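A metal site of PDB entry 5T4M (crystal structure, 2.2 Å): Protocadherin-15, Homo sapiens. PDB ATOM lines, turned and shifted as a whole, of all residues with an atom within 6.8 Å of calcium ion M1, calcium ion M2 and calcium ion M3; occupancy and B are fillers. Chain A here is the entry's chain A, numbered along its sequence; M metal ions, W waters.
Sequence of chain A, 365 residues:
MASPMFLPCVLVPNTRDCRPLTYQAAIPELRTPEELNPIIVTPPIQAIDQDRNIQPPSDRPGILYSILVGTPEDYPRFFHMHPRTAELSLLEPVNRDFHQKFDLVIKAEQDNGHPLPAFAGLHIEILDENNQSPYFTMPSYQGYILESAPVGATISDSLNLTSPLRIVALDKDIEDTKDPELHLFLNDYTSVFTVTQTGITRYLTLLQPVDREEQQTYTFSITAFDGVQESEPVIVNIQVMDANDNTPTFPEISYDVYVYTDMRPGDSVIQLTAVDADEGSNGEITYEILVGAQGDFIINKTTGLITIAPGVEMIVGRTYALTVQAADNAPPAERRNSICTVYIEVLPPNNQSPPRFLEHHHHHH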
ATOM      1  N   GLU A 147     -24.863  36.197   2.247  1.00  0.00           N
ATOM      2  CA  GLU A 147     -26.216  35.825   1.824  1.00  0.00           C
ATOM      3  C   GLU A 147     -27.282  36.166   2.868  1.00  0.00           C
ATOM      4  O   GLU A 147     -28.467  36.256   2.543  1.00  0.00           O
ATOM      5  CB  GLU A 147     -26.282  34.328   1.502  1.00  0.00           C
ATOM      6  CG  GLU A 147     -26.131  33.395   2.696  1.00  0.00           C
ATOM      7  CD  GLU A 147     -26.288  31.935   2.304  1.00  0.00           C
ATOM      8  OE1 GLU A 147     -25.446  31.102   2.691  1.00  0.00           O
ATOM      9  OE2 GLU A 147     -27.269  31.617   1.588  1.00  0.00           O
ATOM     10  N   VAL A 210     -30.316  37.604  -1.418  1.00  0.00           N
ATOM     11  CA  VAL A 210     -29.708  36.587  -2.262  1.00  0.00           C
ATOM     12  C   VAL A 210     -29.450  35.318  -1.461  1.00  0.00           C
ATOM     13  O   VAL A 210     -29.229  35.361  -0.254  1.00  0.00           O
ATOM     14  CB  VAL A 210     -28.381  37.079  -2.897  1.00  0.00           C
ATOM     15  CG1 VAL A 210     -28.672  38.102  -3.980  1.00  0.00           C
ATOM     16  CG2 VAL A 210     -27.460  37.652  -1.836  1.00  0.00           C
ATOM     17  N   ASP A 211     -29.484  34.180  -2.151  1.00  0.00           N
ATOM     18  CA  ASP A 211     -29.320  32.884  -1.523  1.00  0.00           C
ATOM     19  C   ASP A 211     -28.187  32.130  -2.213  1.00  0.00           C
ATOM     20  O   ASP A 211     -28.311  31.717  -3.365  1.00  0.00           O
ATOM     21  CB  ASP A 211     -30.627  32.091  -1.597  1.00  0.00           C
ATOM     22  CG  ASP A 211     -30.532  30.695  -1.006  1.00  0.00           C
ATOM     23  OD1 ASP A 211     -29.566  30.410  -0.264  1.00  0.00           O
ATOM     24  OD2 ASP A 211     -31.426  29.869  -1.278  1.00  0.00           O
ATOM     25  N   ARG A 212     -27.070  31.956  -1.493  1.00  0.00           N
ATOM     26  CA  ARG A 212     -25.897  31.308  -2.057  1.00  0.00           C
ATOM     27  C   ARG A 212     -26.221  29.936  -2.604  1.00  0.00           C
ATOM     28  O   ARG A 212     -25.727  29.547  -3.664  1.00  0.00           O
ATOM     29  CB  ARG A 212     -24.773  31.182  -1.027  1.00  0.00           C
ATOM     30  CG  ARG A 212     -23.434  30.805  -1.654  1.00  0.00           C
ATOM     31  CD  ARG A 212     -22.523  30.057  -0.702  1.00  0.00           C
ATOM     32  NE  ARG A 212     -23.111  28.795  -0.277  1.00  0.00           N
ATOM     33  CZ  ARG A 212     -22.998  27.646  -0.937  1.00  0.00           C
ATOM     34  NH1 ARG A 212     -22.294  27.593  -2.065  1.00  0.00           N
ATOM     35  NH2 ARG A 212     -23.576  26.548  -0.463  1.00  0.00           N
ATOM     36  N   GLU A 213     -27.071  29.204  -1.883  1.00  0.00           N
ATOM     37  CA  GLU A 213     -27.463  27.855  -2.300  1.00  0.00           C
ATOM     38  C   GLU A 213     -28.257  27.881  -3.615  1.00  0.00           C
ATOM     39  O   GLU A 213     -28.372  26.867  -4.302  1.00  0.00           O
ATOM     40  CB  GLU A 213     -28.263  27.158  -1.199  1.00  0.00           C
ATOM     41  CG  GLU A 213     -27.417  26.565  -0.069  1.00  0.00           C
ATOM     42  CD  GLU A 213     -26.760  27.615   0.815  1.00  0.00           C
ATOM     43  OE1 GLU A 213     -27.465  28.513   1.323  1.00  0.00           O
ATOM     44  OE2 GLU A 213     -25.531  27.544   1.018  1.00  0.00           O
ATOM     45  N   GLU A 214     -28.815  29.047  -3.950  1.00  0.00           N
ATOM     46  CA  GLU A 214     -29.554  29.234  -5.191  1.00  0.00           C
ATOM     47  C   GLU A 214     -28.637  29.717  -6.318  1.00  0.00           C
ATOM     48  O   GLU A 214     -28.647  29.158  -7.402  1.00  0.00           O
ATOM     49  CB  GLU A 214     -30.702  30.218  -4.968  1.00  0.00           C
ATOM     50  CG  GLU A 214     -31.799  30.176  -6.017  1.00  0.00           C
ATOM     51  CD  GLU A 214     -32.988  31.042  -5.647  1.00  0.00           C
ATOM     52  OE1 GLU A 214     -32.782  32.167  -5.146  1.00  0.00           O
ATOM     53  OE2 GLU A 214     -34.137  30.596  -5.855  1.00  0.00           O
ATOM     54  N   MET A 241     -21.435  35.147  -0.285  1.00  0.00           N
ATOM     55  CA  MET A 241     -20.724  34.363   0.725  1.00  0.00           C
ATOM     56  C   MET A 241     -21.659  33.542   1.604  1.00  0.00           C
ATOM     57  O   MET A 241     -22.775  33.976   1.929  1.00  0.00           O
ATOM     58  CB  MET A 241     -19.855  35.293   1.580  1.00  0.00           C
ATOM     59  CG  MET A 241     -18.759  35.992   0.782  1.00  0.00           C
ATOM     60  SD  MET A 241     -17.808  37.174   1.751  1.00  0.00           S
ATOM     61  CE  MET A 241     -16.885  36.085   2.827  1.00  0.00           C
ATOM     62  N   ASP A 242     -21.201  32.362   1.983  1.00  0.00           N
ATOM     63  CA  ASP A 242     -22.035  31.392   2.693  1.00  0.00           C
ATOM     64  C   ASP A 242     -22.337  31.792   4.124  1.00  0.00           C
ATOM     65  O   ASP A 242     -21.456  32.222   4.871  1.00  0.00           O
ATOM     66  CB  ASP A 242     -21.359  30.014   2.676  1.00  0.00           C
ATOM     67  CG  ASP A 242     -22.274  28.910   3.181  1.00  0.00           C
ATOM     68  OD1 ASP A 242     -23.466  28.890   2.808  1.00  0.00           O
ATOM     69  OD2 ASP A 242     -21.798  28.055   3.959  1.00  0.00           O
ATOM     70  N   ALA A 243     -23.613  31.680   4.489  1.00  0.00           N
ATOM     71  CA  ALA A 243     -24.016  31.673   5.887  1.00  0.00           C
ATOM     72  C   ALA A 243     -24.455  30.263   6.229  1.00  0.00           C
ATOM     73  O   ALA A 243     -24.971  29.545   5.371  1.00  0.00           O
ATOM     74  CB  ALA A 243     -25.132  32.665   6.136  1.00  0.00           C
ATOM     75  N   ASN A 244     -24.254  29.852   7.475  1.00  0.00           N
ATOM     76  CA  ASN A 244     -24.750  28.543   7.893  1.00  0.00           C
ATOM     77  C   ASN A 244     -26.246  28.616   8.140  1.00  0.00           C
ATOM     78  O   ASN A 244     -26.694  28.701   9.288  1.00  0.00           O
ATOM     79  CB  ASN A 244     -24.025  28.061   9.160  1.00  0.00           C
ATOM     80  CG  ASN A 244     -24.243  26.582   9.407  1.00  0.00           C
ATOM     81  OD1 ASN A 244     -24.251  25.781   8.475  1.00  0.00           O
ATOM     82  ND2 ASN A 244     -24.447  26.209  10.667  1.00  0.00           N
ATOM     83  N   ASP A 245     -27.005  28.608   7.046  1.00  0.00           N
ATOM     84  CA  ASP A 245     -28.455  28.735   7.113  1.00  0.00           C
ATOM     85  C   ASP A 245     -29.144  27.480   6.597  1.00  0.00           C
ATOM     86  O   ASP A 245     -30.324  27.507   6.240  1.00  0.00           O
ATOM     87  CB  ASP A 245     -28.924  29.997   6.354  1.00  0.00           C
ATOM     88  CG  ASP A 245     -28.823  29.871   4.825  1.00  0.00           C
ATOM     89  OD1 ASP A 245     -27.998  29.103   4.281  1.00  0.00           O
ATOM     90  OD2 ASP A 245     -29.587  30.596   4.153  1.00  0.00           O
ATOM     91  N   ASN A 246     -28.401  26.378   6.568  1.00  0.00           N
ATOM     92  CA  ASN A 246     -28.969  25.055   6.311  1.00  0.00           C
ATOM     93  C   ASN A 246     -28.588  24.045   7.403  1.00  0.00           C
ATOM     94  O   ASN A 246     -27.447  23.976   7.833  1.00  0.00           O
ATOM     95  CB  ASN A 246     -28.519  24.527   4.952  1.00  0.00           C
ATOM     96  CG  ASN A 246     -29.229  25.216   3.812  1.00  0.00           C
ATOM     97  OD1 ASN A 246     -30.221  24.704   3.288  1.00  0.00           O
ATOM     98  ND2 ASN A 246     -28.746  26.401   3.427  1.00  0.00           N
ATOM     99  N   THR A 247     -29.584  23.276   7.828  1.00  0.00           N
ATOM    100  CA  THR A 247     -29.424  22.307   8.904  1.00  0.00           C
ATOM    101  C   THR A 247     -29.225  20.905   8.337  1.00  0.00           C
ATOM    102  O   THR A 247     -29.916  20.514   7.405  1.00  0.00           O
ATOM    103  CB  THR A 247     -30.656  22.322   9.840  1.00  0.00           C
ATOM    104  OG1 THR A 247     -30.735  23.584  10.512  1.00  0.00           O
ATOM    105  CG2 THR A 247     -30.604  21.202  10.874  1.00  0.00           C
ATOM    106  N   PRO A 248     -28.255  20.145   8.889  1.00  0.00           N
ATOM    107  CA  PRO A 248     -28.076  18.749   8.481  1.00  0.00           C
ATOM    108  C   PRO A 248     -29.386  17.976   8.611  1.00  0.00           C
ATOM    109  O   PRO A 248     -29.986  17.971   9.684  1.00  0.00           O
ATOM    110  CB  PRO A 248     -27.027  18.220   9.467  1.00  0.00           C
ATOM    111  CG  PRO A 248     -26.267  19.430   9.878  1.00  0.00           C
ATOM    112  CD  PRO A 248     -27.263  20.565   9.891  1.00  0.00           C
ATOM    113  N   ASP A 276     -26.593  18.568   4.017  1.00  0.00           N
ATOM    114  CA  ASP A 276     -26.381  19.968   4.366  1.00  0.00           C
ATOM    115  C   ASP A 276     -25.854  20.698   3.126  1.00  0.00           C
ATOM    116  O   ASP A 276     -24.806  20.339   2.592  1.00  0.00           O
ATOM    117  CB  ASP A 276     -25.405  20.093   5.540  1.00  0.00           C
ATOM    118  CG  ASP A 276     -25.455  21.463   6.212  1.00  0.00           C
ATOM    119  OD1 ASP A 276     -25.348  22.499   5.519  1.00  0.00           O
ATOM    120  OD2 ASP A 276     -25.603  21.490   7.451  1.00  0.00           O
ATOM    121  N   ALA A 277     -26.591  21.703   2.658  1.00  0.00           N
ATOM    122  CA  ALA A 277     -26.288  22.361   1.386  1.00  0.00           C
ATOM    123  C   ALA A 277     -25.294  23.512   1.531  1.00  0.00           C
ATOM    124  O   ALA A 277     -24.897  24.107   0.534  1.00  0.00           O
ATOM    125  CB  ALA A 277     -27.577  22.859   0.747  1.00  0.00           C
ATOM    126  N   ASP A 278     -24.904  23.822   2.757  1.00  0.00           N
ATOM    127  CA  ASP A 278     -23.996  24.934   2.999  1.00  0.00           C
ATOM    128  C   ASP A 278     -22.582  24.623   2.487  1.00  0.00           C
ATOM    129  O   ASP A 278     -22.289  23.487   2.096  1.00  0.00           O
ATOM    130  CB  ASP A 278     -23.957  25.278   4.488  1.00  0.00           C
ATOM    131  CG  ASP A 278     -25.263  25.858   4.977  1.00  0.00           C
ATOM    132  OD1 ASP A 278     -25.888  26.647   4.241  1.00  0.00           O
ATOM    133  OD2 ASP A 278     -25.683  25.512   6.102  1.00  0.00           O
ATOM    134  N   GLU A 279     -21.722  25.628   2.508  1.00  0.00           N
ATOM    135  CA  GLU A 279     -20.397  25.516   1.904  1.00  0.00           C
ATOM    136  C   GLU A 279     -19.329  25.152   2.935  1.00  0.00           C
ATOM    137  O   GLU A 279     -19.362  25.614   4.067  1.00  0.00           O
ATOM    138  CB  GLU A 279     -20.031  26.831   1.215  1.00  0.00           C
ATOM    139  CG  GLU A 279     -18.842  26.761   0.286  1.00  0.00           C
ATOM    140  CD  GLU A 279     -18.556  28.075  -0.413  1.00  0.00           C
ATOM    141  OE1 GLU A 279     -18.127  28.055  -1.582  1.00  0.00           O
ATOM    142  OE2 GLU A 279     -18.772  29.146   0.212  1.00  0.00           O
ATOM    143  N   SER A 281     -17.052  23.861   5.751  1.00  0.00           N
ATOM    144  CA  SER A 281     -17.290  23.316   7.080  1.00  0.00           C
ATOM    145  C   SER A 281     -18.729  23.565   7.539  1.00  0.00           C
ATOM    146  O   SER A 281     -19.227  22.860   8.424  1.00  0.00           O
ATOM    147  CB  SER A 281     -16.300  23.921   8.085  1.00  0.00           C
ATOM    148  OG  SER A 281     -16.544  25.302   8.288  1.00  0.00           O
ATOM    149  N   ASN A 282     -19.389  24.549   6.937  1.00  0.00           N
ATOM    150  CA  ASN A 282     -20.798  24.801   7.213  1.00  0.00           C
ATOM    151  C   ASN A 282     -21.681  23.668   6.693  1.00  0.00           C
ATOM    152  O   ASN A 282     -22.795  23.452   7.171  1.00  0.00           O
ATOM    153  CB  ASN A 282     -21.252  26.134   6.613  1.00  0.00           C
ATOM    154  CG  ASN A 282     -20.722  27.332   7.376  1.00  0.00           C
ATOM    155  OD1 ASN A 282     -20.357  27.232   8.541  1.00  0.00           O
ATOM    156  ND2 ASN A 282     -20.706  28.491   6.714  1.00  0.00           N
ATOM    157  N   GLY A 283     -21.165  22.939   5.704  1.00  0.00           N
ATOM    158  CA  GLY A 283     -21.864  21.799   5.151  1.00  0.00           C
ATOM    159  C   GLY A 283     -21.264  20.468   5.581  1.00  0.00           C
ATOM    160  O   GLY A 283     -21.806  19.402   5.263  1.00  0.00           O
ATOM    161  N   GLU A 284     -20.142  20.529   6.288  1.00  0.00           N
ATOM    162  CA  GLU A 284     -19.449  19.333   6.749  1.00  0.00           C
ATOM    163  C   GLU A 284     -20.180  18.678   7.920  1.00  0.00           C
ATOM    164  O   GLU A 284     -20.303  19.272   8.990  1.00  0.00           O
ATOM    165  CB  GLU A 284     -18.012  19.685   7.157  1.00  0.00           C
ATOM    166  CG  GLU A 284     -17.161  18.506   7.583  1.00  0.00           C
ATOM    167  CD  GLU A 284     -15.775  18.923   8.048  1.00  0.00           C
ATOM    168  OE1 GLU A 284     -15.438  20.125   7.913  1.00  0.00           O
ATOM    169  OE2 GLU A 284     -15.026  18.060   8.540  1.00  0.00           O
ATOM    170  N   ASP A 328     -23.383  20.006  11.720  1.00  0.00           N
ATOM    171  CA  ASP A 328     -22.379  20.570  10.819  1.00  0.00           C
ATOM    172  C   ASP A 328     -21.197  21.105  11.610  1.00  0.00           C
ATOM    173  O   ASP A 328     -21.285  21.281  12.829  1.00  0.00           O
ATOM    174  CB  ASP A 328     -22.977  21.664   9.911  1.00  0.00           C
ATOM    175  CG  ASP A 328     -23.728  22.747  10.675  1.00  0.00           C
ATOM    176  OD1 ASP A 328     -23.368  23.057  11.831  1.00  0.00           O
ATOM    177  OD2 ASP A 328     -24.683  23.301  10.091  1.00  0.00           O
ATOM    178  N   ASN A 329     -20.086  21.346  10.928  1.00  0.00           N
ATOM    179  CA  ASN A 329     -18.868  21.782  11.594  1.00  0.00           C
ATOM    180  C   ASN A 329     -18.629  23.287  11.482  1.00  0.00           C
ATOM    181  O   ASN A 329     -17.500  23.737  11.289  1.00  0.00           O
ATOM    182  CB  ASN A 329     -17.662  21.017  11.044  1.00  0.00           C
ATOM    183  CG  ASN A 329     -17.493  19.667  11.718  1.00  0.00           C
ATOM    184  OD1 ASN A 329     -18.046  18.662  11.264  1.00  0.00           O
ATOM    185  ND2 ASN A 329     -16.732  19.636  12.803  1.00  0.00           N
ATOM    186  N   ALA A 330     -19.713  24.040  11.601  1.00  0.00           N
ATOM    187  CA  ALA A 330     -19.612  25.477  11.781  1.00  0.00           C
ATOM    188  C   ALA A 330     -19.148  25.727  13.208  1.00  0.00           C
ATOM    189  O   ALA A 330     -19.234  24.844  14.047  1.00  0.00           O
ATOM    190  CB  ALA A 330     -20.960  26.141  11.517  1.00  0.00           C
ATOM    191  N   GLU A 334     -22.774  29.024  15.638  1.00  0.00           N
ATOM    192  CA  GLU A 334     -23.629  28.961  14.458  1.00  0.00           C
ATOM    193  C   GLU A 334     -23.991  27.535  14.062  1.00  0.00           C
ATOM    194  O   GLU A 334     -24.679  27.316  13.064  1.00  0.00           O
ATOM    195  CB  GLU A 334     -22.953  29.658  13.273  1.00  0.00           C
ATOM    196  CG  GLU A 334     -22.614  31.124  13.505  1.00  0.00           C
ATOM    197  CD  GLU A 334     -21.125  31.333  13.686  1.00  0.00           C
ATOM    198  OE1 GLU A 334     -20.606  31.082  14.802  1.00  0.00           O
ATOM    199  OE2 GLU A 334     -20.461  31.749  12.715  1.00  0.00           O
ATOM    200  N   ARG A 336     -25.518  23.914  13.526  1.00  0.00           N
ATOM    201  CA  ARG A 336     -26.871  23.386  13.405  1.00  0.00           C
ATOM    202  C   ARG A 336     -26.856  21.858  13.440  1.00  0.00           C
ATOM    203  O   ARG A 336     -25.906  21.233  12.975  1.00  0.00           O
ATOM    204  CB  ARG A 336     -27.529  23.864  12.115  1.00  0.00           C
ATOM    205  CG  ARG A 336     -27.917  25.323  12.112  1.00  0.00           C
ATOM    206  CD  ARG A 336     -28.329  25.776  10.724  1.00  0.00           C
ATOM    207  NE  ARG A 336     -28.835  27.151  10.752  1.00  0.00           N
ATOM    208  CZ  ARG A 336     -30.132  27.457  10.718  1.00  0.00           C
ATOM    209  NH1 ARG A 336     -31.038  26.495  10.631  1.00  0.00           N
ATOM    210  NH2 ARG A 336     -30.510  28.733  10.756  1.00  0.00           N
HETATM  211 CA    CA M   1     -25.118  23.758   7.612  1.00  0.00          CA
HETATM  212 CA    CA M   2     -25.785  28.750   3.218  1.00  0.00          CA
HETATM  213 CA    CA M   3     -28.979  30.094   1.951  1.00  0.00          CA
HETATM  214  O   HOH W   1     -30.609  28.256   2.199  1.00  0.00           O
HETATM  215  O   HOH W   2     -30.516  31.780   1.803  1.00  0.00           O
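Seven residues have an atom within 4 Å of calcium ion M2: Glu 147, Glu 213, Asp 242, Ala 243, Asp 245, Asn 246 and Asp 278.
Along chain A the residues within 4 Å of calcium ion M2 span positions 147 to 278.
The nearest printed residue that does not touch calcium ion M2 is Arg 212 (4.4 Å).
The side-chain carboxylate of Asp 242 lies within hydrogen-bond range of the side-chain amide nitrogen of Asn 282 (3.0 Å).
NE of Arg 212 lies close to OD1 of Asp 242, at 3.1 Å.
The side-chain carboxylate (OE2) of Glu 213 sits close to the guanidinium group (NH2) of Arg 212, 2.6 Å away.
ND2 of Asn 246 lies close to OE1 of Glu 213 (3.2 Å).
The backbone carbonyl oxygen (O) of Asn 244 sits at hydrogen-bond distance from the guanidinium group (NE) of Arg 336 (3.0 Å).
OD1 of Asp 245 sits close to ND2 of Asn 246 (2.9 Å).
The backbone NH (N) of Arg 212 sits close to the side-chain carboxylate (OE2) of Glu 147 (3.1 Å).
The side-chain carboxylate (OD1) of Asp 328 sits at hydrogen-bond distance from the backbone NH (N) of Arg 336.
Calcium ion M2 is bound by OD1 of Asp 278 (2.3 Å), OD1 of Asp 242 (2.4 Å), OE1 of Glu 147 (2.4 Å), O of Ala 243 (2.4 Å), OD1 of Asp 245 (2.5 Å), OE2 of Glu 213 (2.5 Å) and OE1 of Glu 213 (2.5 Å).
Within 4 Å of calcium ion M3: Glu 147, Asp 211, Glu 213, Asp 245 and Asn 246.
The side-chain carboxylate (OE1) of Glu 213 is bound to calcium ion M3, 2.3 Å away.
Water W2 binds calcium ion M3, at 2.3 Å.
OD1 of Asp 211 binds calcium ion M3.
OE2 of Glu 147 is bound to calcium ion M3 (2.3 Å).
Calcium ion M3 is bound by OD2 of Asp 245, at 2.3 Å.
Water W1 is bound to calcium ion M3, 2.5 Å away.
Calcium ion M3 is bound by OD1 of Asp 245, 2.7 Å away.
Calcium ion M1 is bound by OD2 of Asp 276 (2.3 Å), O of Asn 246 (2.3 Å), OD1 of Asn 244 (2.4 Å), OD2 of Asp 278 (2.4 Å), O of Asn 282 (2.4 Å), OD1 of Asp 276 (2.5 Å) and OD2 of Asp 328 (2.6 Å).
Calcium ion M1 has seven donor atoms within binding distance.
Within 4 Å of calcium ion M1: Asn 244, Asn 246, Asp 276, Asp 278, Asn 282 and Asp 328.
Along chain A the residues within 4 Å of calcium ion M1 span positions 244 to 328.
The nearest printed residue that does not touch calcium ion M1 is Gly 283 (4.5 Å).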
